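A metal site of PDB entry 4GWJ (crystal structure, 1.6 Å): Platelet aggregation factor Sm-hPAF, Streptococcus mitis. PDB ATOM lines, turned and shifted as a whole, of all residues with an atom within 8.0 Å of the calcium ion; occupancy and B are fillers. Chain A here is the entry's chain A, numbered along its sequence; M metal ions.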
ATOM      1  N   ALA A  28      21.923 -24.447  10.470  1.00  0.00           N
ATOM      2  CA  ALA A  28      23.298 -24.800  10.710  1.00  0.00           C
ATOM      3  C   ALA A  28      23.505 -25.719  11.927  1.00  0.00           C
ATOM      4  O   ALA A  28      22.840 -25.468  12.991  1.00  0.00           O
ATOM      5  CB  ALA A  28      24.081 -23.479  10.958  1.00  0.00           C
ATOM      6  N   ALA A  29      24.365 -26.666  11.761  1.00  0.00           N
ATOM      7  CA  ALA A  29      24.676 -27.678  12.830  1.00  0.00           C
ATOM      8  C   ALA A  29      25.084 -26.956  14.094  1.00  0.00           C
ATOM      9  O   ALA A  29      24.799 -27.427  15.252  1.00  0.00           O
ATOM     10  CB  ALA A  29      25.784 -28.649  12.472  1.00  0.00           C
ATOM     11  N   THR A  30      25.741 -25.806  14.049  1.00  0.00           N
ATOM     12  CA  THR A  30      26.218 -25.087  15.248  1.00  0.00           C
ATOM     13  C   THR A  30      25.062 -24.506  16.093  1.00  0.00           C
ATOM     14  O   THR A  30      25.298 -24.166  17.254  1.00  0.00           O
ATOM     15  CB  THR A  30      27.220 -23.982  14.889  1.00  0.00           C
ATOM     16  OG1 THR A  30      26.716 -23.200  13.818  1.00  0.00           O
ATOM     17  CG2 THR A  30      28.469 -24.664  14.406  1.00  0.00           C
ATOM     18  N   ARG A  31      23.853 -24.511  15.575  1.00  0.00           N
ATOM     19  CA  ARG A  31      22.733 -24.019  16.337  1.00  0.00           C
ATOM     20  C   ARG A  31      22.436 -24.947  17.496  1.00  0.00           C
ATOM     21  O   ARG A  31      21.788 -24.548  18.421  1.00  0.00           O
ATOM     22  CB  ARG A  31      21.504 -23.862  15.471  1.00  0.00           C
ATOM     23  CG  ARG A  31      21.597 -22.734  14.464  1.00  0.00           C
ATOM     24  CD  ARG A  31      20.445 -22.709  13.502  1.00  0.00           C
ATOM     25  NE  ARG A  31      20.546 -21.587  12.587  1.00  0.00           N
ATOM     26  CZ  ARG A  31      19.561 -21.162  11.841  1.00  0.00           C
ATOM     27  NH1 ARG A  31      19.734 -20.113  11.070  1.00  0.00           N
ATOM     28  NH2 ARG A  31      18.392 -21.780  11.875  1.00  0.00           N
ATOM     29  N   ALA A  32      22.891 -26.177  17.429  1.00  0.00           N
ATOM     30  CA  ALA A  32      22.583 -27.076  18.637  1.00  0.00           C
ATOM     31  C   ALA A  32      23.616 -26.924  19.709  1.00  0.00           C
ATOM     32  O   ALA A  32      23.478 -27.517  20.844  1.00  0.00           O
ATOM     33  CB  ALA A  32      22.462 -28.553  18.187  1.00  0.00           C
ATOM     34  N   VAL A  33      24.656 -26.130  19.517  1.00  0.00           N
ATOM     35  CA  VAL A  33      25.675 -25.882  20.545  1.00  0.00           C
ATOM     36  C   VAL A  33      25.950 -24.379  20.763  1.00  0.00           C
ATOM     37  O   VAL A  33      26.994 -23.946  21.263  1.00  0.00           O
ATOM     38  CB  VAL A  33      26.994 -26.666  20.318  1.00  0.00           C
ATOM     39  CG1 VAL A  33      26.739 -28.173  20.422  1.00  0.00           C
ATOM     40  CG2 VAL A  33      27.605 -26.328  18.927  1.00  0.00           C
ATOM     41  N   ASP A  34      24.927 -23.559  20.564  1.00  0.00           N
ATOM     42  CA  ASP A  34      25.036 -22.106  20.680  1.00  0.00           C
ATOM     43  C   ASP A  34      24.641 -21.597  22.016  1.00  0.00           C
ATOM     44  O   ASP A  34      24.602 -20.377  22.208  1.00  0.00           O
ATOM     45  CB  ASP A  34      24.308 -21.381  19.546  1.00  0.00           C
ATOM     46  CG  ASP A  34      22.830 -21.519  19.531  1.00  0.00           C
ATOM     47  OD1 ASP A  34      22.264 -22.282  20.429  1.00  0.00           O
ATOM     48  OD2 ASP A  34      22.089 -20.910  18.713  1.00  0.00           O
ATOM     49  N   GLY A  35      24.275 -22.519  22.928  1.00  0.00           N
ATOM     50  CA  GLY A  35      23.931 -21.968  24.215  1.00  0.00           C
ATOM     51  C   GLY A  35      22.524 -21.479  24.374  1.00  0.00           C
ATOM     52  O   GLY A  35      22.244 -20.709  25.333  1.00  0.00           O
ATOM     53  N   ASN A  36      21.621 -21.871  23.488  1.00  0.00           N
ATOM     54  CA  ASN A  36      20.286 -21.353  23.499  1.00  0.00           C
ATOM     55  C   ASN A  36      19.335 -22.457  23.172  1.00  0.00           C
ATOM     56  O   ASN A  36      19.304 -23.131  22.084  1.00  0.00           O
ATOM     57  CB  ASN A  36      20.168 -20.279  22.346  1.00  0.00           C
ATOM     58  CG  ASN A  36      18.835 -19.622  22.321  1.00  0.00           C
ATOM     59  OD1 ASN A  36      17.860 -20.058  22.969  1.00  0.00           O
ATOM     60  ND2 ASN A  36      18.709 -18.634  21.466  1.00  0.00           N
ATOM     61  N   VAL A  37      18.528 -22.965  24.192  1.00  0.00           N
ATOM     62  CA  VAL A  37      17.653 -24.024  23.963  1.00  0.00           C
ATOM     63  C   VAL A  37      16.255 -23.710  23.426  1.00  0.00           C
ATOM     64  O   VAL A  37      15.375 -24.561  23.303  1.00  0.00           O
ATOM     65  CB  VAL A  37      17.418 -24.826  25.349  1.00  0.00           C
ATOM     66  CG1 VAL A  37      18.753 -25.264  25.958  1.00  0.00           C
ATOM     67  CG2 VAL A  37      16.603 -23.983  26.380  1.00  0.00           C
ATOM     68  N   ASP A  38      16.084 -22.443  23.032  1.00  0.00           N
ATOM     69  CA  ASP A  38      14.828 -22.026  22.405  1.00  0.00           C
ATOM     70  C   ASP A  38      14.419 -22.922  21.274  1.00  0.00           C
ATOM     71  O   ASP A  38      15.196 -23.091  20.299  1.00  0.00           O
ATOM     72  CB  ASP A  38      14.931 -20.587  21.911  1.00  0.00           C
ATOM     73  CG  ASP A  38      13.616 -20.022  21.465  1.00  0.00           C
ATOM     74  OD1 ASP A  38      13.487 -18.717  21.627  1.00  0.00           O
ATOM     75  OD2 ASP A  38      12.717 -20.645  20.929  1.00  0.00           O
ATOM     76  N   SER A  39      13.268 -23.589  21.408  1.00  0.00           N
ATOM     77  CA  SER A  39      12.890 -24.617  20.466  1.00  0.00           C
ATOM     78  C   SER A  39      12.080 -24.208  19.269  1.00  0.00           C
ATOM     79  O   SER A  39      11.676 -25.044  18.449  1.00  0.00           O
ATOM     80  CB  SER A  39      12.182 -25.744  21.250  1.00  0.00           C
ATOM     81  OG  SER A  39      10.922 -25.237  21.650  1.00  0.00           O
ATOM     82  N   HIS A  43      13.161 -18.766  15.749  1.00  0.00           N
ATOM     83  CA  HIS A  43      14.079 -17.962  16.519  1.00  0.00           C
ATOM     84  C   HIS A  43      15.576 -18.305  16.264  1.00  0.00           C
ATOM     85  O   HIS A  43      16.468 -17.841  16.965  1.00  0.00           O
ATOM     86  CB  HIS A  43      13.728 -18.190  17.987  1.00  0.00           C
ATOM     87  CG  HIS A  43      12.366 -17.674  18.293  1.00  0.00           C
ATOM     88  ND1 HIS A  43      11.789 -17.948  19.547  1.00  0.00           N
ATOM     89  CD2 HIS A  43      11.435 -17.007  17.563  1.00  0.00           C
ATOM     90  CE1 HIS A  43      10.514 -17.437  19.537  1.00  0.00           C
ATOM     91  NE2 HIS A  43      10.287 -16.858  18.357  1.00  0.00           N
ATOM     92  N   HIS A  44      15.799 -19.181  15.211  1.00  0.00           N
ATOM     93  CA  HIS A  44      17.121 -19.437  14.602  1.00  0.00           C
ATOM     94  C   HIS A  44      18.118 -20.242  15.382  1.00  0.00           C
ATOM     95  O   HIS A  44      19.326 -20.194  15.209  1.00  0.00           O
ATOM     96  CB  HIS A  44      17.840 -18.092  14.226  1.00  0.00           C
ATOM     97  CG  HIS A  44      16.977 -17.164  13.455  1.00  0.00           C
ATOM     98  ND1 HIS A  44      16.412 -17.503  12.281  1.00  0.00           N
ATOM     99  CD2 HIS A  44      16.647 -15.848  13.724  1.00  0.00           C
ATOM    100  CE1 HIS A  44      15.697 -16.364  11.838  1.00  0.00           C
ATOM    101  NE2 HIS A  44      15.851 -15.406  12.723  1.00  0.00           N
ATOM    102  N   SER A  45      17.602 -20.924  16.461  1.00  0.00           N
ATOM    103  CA  SER A  45      18.549 -21.702  17.305  1.00  0.00           C
ATOM    104  C   SER A  45      18.314 -23.231  17.198  1.00  0.00           C
ATOM    105  O   SER A  45      18.728 -23.988  18.087  1.00  0.00           O
ATOM    106  CB  SER A  45      18.503 -21.207  18.816  1.00  0.00           C
ATOM    107  OG  SER A  45      19.698 -21.578  19.446  1.00  0.00           O
ATOM    108  N   VAL A  46      17.671 -23.683  16.108  1.00  0.00           N
ATOM    109  CA  VAL A  46      17.368 -25.092  15.927  1.00  0.00           C
ATOM    110  C   VAL A  46      18.003 -25.538  14.614  1.00  0.00           C
ATOM    111  O   VAL A  46      17.901 -24.803  13.587  1.00  0.00           O
ATOM    112  CB  VAL A  46      15.839 -25.321  15.868  1.00  0.00           C
ATOM    113  CG1 VAL A  46      15.439 -26.810  15.582  1.00  0.00           C
ATOM    114  CG2 VAL A  46      15.131 -24.761  17.216  1.00  0.00           C
ATOM    115  N   THR A  47      18.588 -26.728  14.650  1.00  0.00           N
ATOM    116  CA  THR A  47      19.275 -27.230  13.400  1.00  0.00           C
ATOM    117  C   THR A  47      18.244 -27.828  12.422  1.00  0.00           C
ATOM    118  O   THR A  47      17.052 -28.040  12.784  1.00  0.00           O
ATOM    119  CB  THR A  47      20.264 -28.348  13.732  1.00  0.00           C
ATOM    120  OG1 THR A  47      19.530 -29.507  14.234  1.00  0.00           O
ATOM    121  CG2 THR A  47      21.327 -27.944  14.813  1.00  0.00           C
ATOM    122  N   TYR A  73      17.459 -31.387  23.352  1.00  0.00           N
ATOM    123  CA  TYR A  73      16.299 -30.487  23.429  1.00  0.00           C
ATOM    124  C   TYR A  73      15.688 -30.491  22.071  1.00  0.00           C
ATOM    125  O   TYR A  73      16.374 -30.183  21.045  1.00  0.00           O
ATOM    126  CB  TYR A  73      16.702 -29.038  23.797  1.00  0.00           C
ATOM    127  CG  TYR A  73      17.301 -28.890  25.167  1.00  0.00           C
ATOM    128  CD1 TYR A  73      16.466 -28.342  26.197  1.00  0.00           C
ATOM    129  CD2 TYR A  73      18.561 -29.351  25.483  1.00  0.00           C
ATOM    130  CE1 TYR A  73      17.043 -28.150  27.424  1.00  0.00           C
ATOM    131  CE2 TYR A  73      19.112 -29.224  26.773  1.00  0.00           C
ATOM    132  CZ  TYR A  73      18.288 -28.647  27.710  1.00  0.00           C
ATOM    133  OH  TYR A  73      18.810 -28.412  28.967  1.00  0.00           O
ATOM    134  N   LEU A 138      17.537 -30.307  15.975  1.00  0.00           N
ATOM    135  CA  LEU A 138      17.748 -30.305  17.457  1.00  0.00           C
ATOM    136  C   LEU A 138      17.801 -28.886  17.886  1.00  0.00           C
ATOM    137  O   LEU A 138      18.522 -28.016  17.274  1.00  0.00           O
ATOM    138  CB  LEU A 138      19.062 -31.024  17.748  1.00  0.00           C
ATOM    139  CG  LEU A 138      19.053 -32.465  17.373  1.00  0.00           C
ATOM    140  CD1 LEU A 138      20.452 -32.970  17.265  1.00  0.00           C
ATOM    141  CD2 LEU A 138      18.430 -33.216  18.582  1.00  0.00           C
ATOM    142  N   ALA A 139      17.120 -28.484  18.963  1.00  0.00           N
ATOM    143  CA  ALA A 139      17.282 -27.134  19.455  1.00  0.00           C
ATOM    144  C   ALA A 139      18.583 -26.947  20.187  1.00  0.00           C
ATOM    145  O   ALA A 139      19.169 -25.894  20.226  1.00  0.00           O
ATOM    146  CB  ALA A 139      16.095 -26.795  20.453  1.00  0.00           C
ATOM    147  N   GLU A 140      19.059 -28.023  20.874  1.00  0.00           N
ATOM    148  CA  GLU A 140      20.350 -27.894  21.579  1.00  0.00           C
ATOM    149  C   GLU A 140      20.727 -29.330  21.998  1.00  0.00           C
ATOM    150  O   GLU A 140      19.817 -30.182  22.208  1.00  0.00           O
ATOM    151  CB  GLU A 140      20.211 -26.973  22.853  1.00  0.00           C
ATOM    152  CG  GLU A 140      21.518 -26.546  23.480  1.00  0.00           C
ATOM    153  CD  GLU A 140      22.288 -25.380  22.783  1.00  0.00           C
ATOM    154  OE1 GLU A 140      21.725 -24.965  21.776  1.00  0.00           O
ATOM    155  OE2 GLU A 140      23.333 -25.042  23.293  1.00  0.00           O
ATOM    156  N   VAL A 141      22.037 -29.535  22.051  1.00  0.00           N
ATOM    157  CA  VAL A 141      22.575 -30.776  22.692  1.00  0.00           C
ATOM    158  C   VAL A 141      23.603 -30.310  23.670  1.00  0.00           C
ATOM    159  O   VAL A 141      24.536 -29.588  23.412  1.00  0.00           O
ATOM    160  CB  VAL A 141      23.250 -31.682  21.631  1.00  0.00           C
ATOM    161  CG1 VAL A 141      23.962 -32.826  22.343  1.00  0.00           C
ATOM    162  CG2 VAL A 141      22.282 -32.135  20.541  1.00  0.00           C
HETATM  163 CA    CA M   1      20.299 -23.840  20.117  1.00  0.00          CA
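N of Asp 38 sits at hydrogen-bond distance from OD1 of Asn 36 (3.0 Å).
O of Tyr 73 is in hydrogen-bond range of N of Ala 139, 2.8 Å away.
The backbone carbonyl oxygen (O) of His 44 lies within hydrogen-bond range of the guanidinium group (NE) of Arg 31, 3.2 Å away.
The side-chain carboxylate of Glu 140 sits at hydrogen-bond distance from the backbone NH of Gly 35, at 2.7 Å.
The backbone carbonyl oxygen (O) of Glu 140 sits at hydrogen-bond distance from the backbone NH (N) of Tyr 73 (2.9 Å).
Within 4 Å of the calcium ion: Arg 31, Asp 34, Asn 36, Ser 45, Ala 139 and Glu 140.
The backbone carbonyl oxygen (O) of Asn 36 is bound to the calcium ion (2.3 Å).
O of Ala 139 binds the calcium ion.
The backbone carbonyl oxygen (O) of Arg 31 is bound to the calcium ion, 2.4 Å away.
The calcium ion is bound by OG of Ser 45 (2.4 Å).
The calcium ion is bound by OE1 of Glu 140 (2.5 Å).
OD1 of Asp 34 binds the calcium ion, 2.5 Å away.
The calcium ion is bound by O of Ser 45 (2.6 Å).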
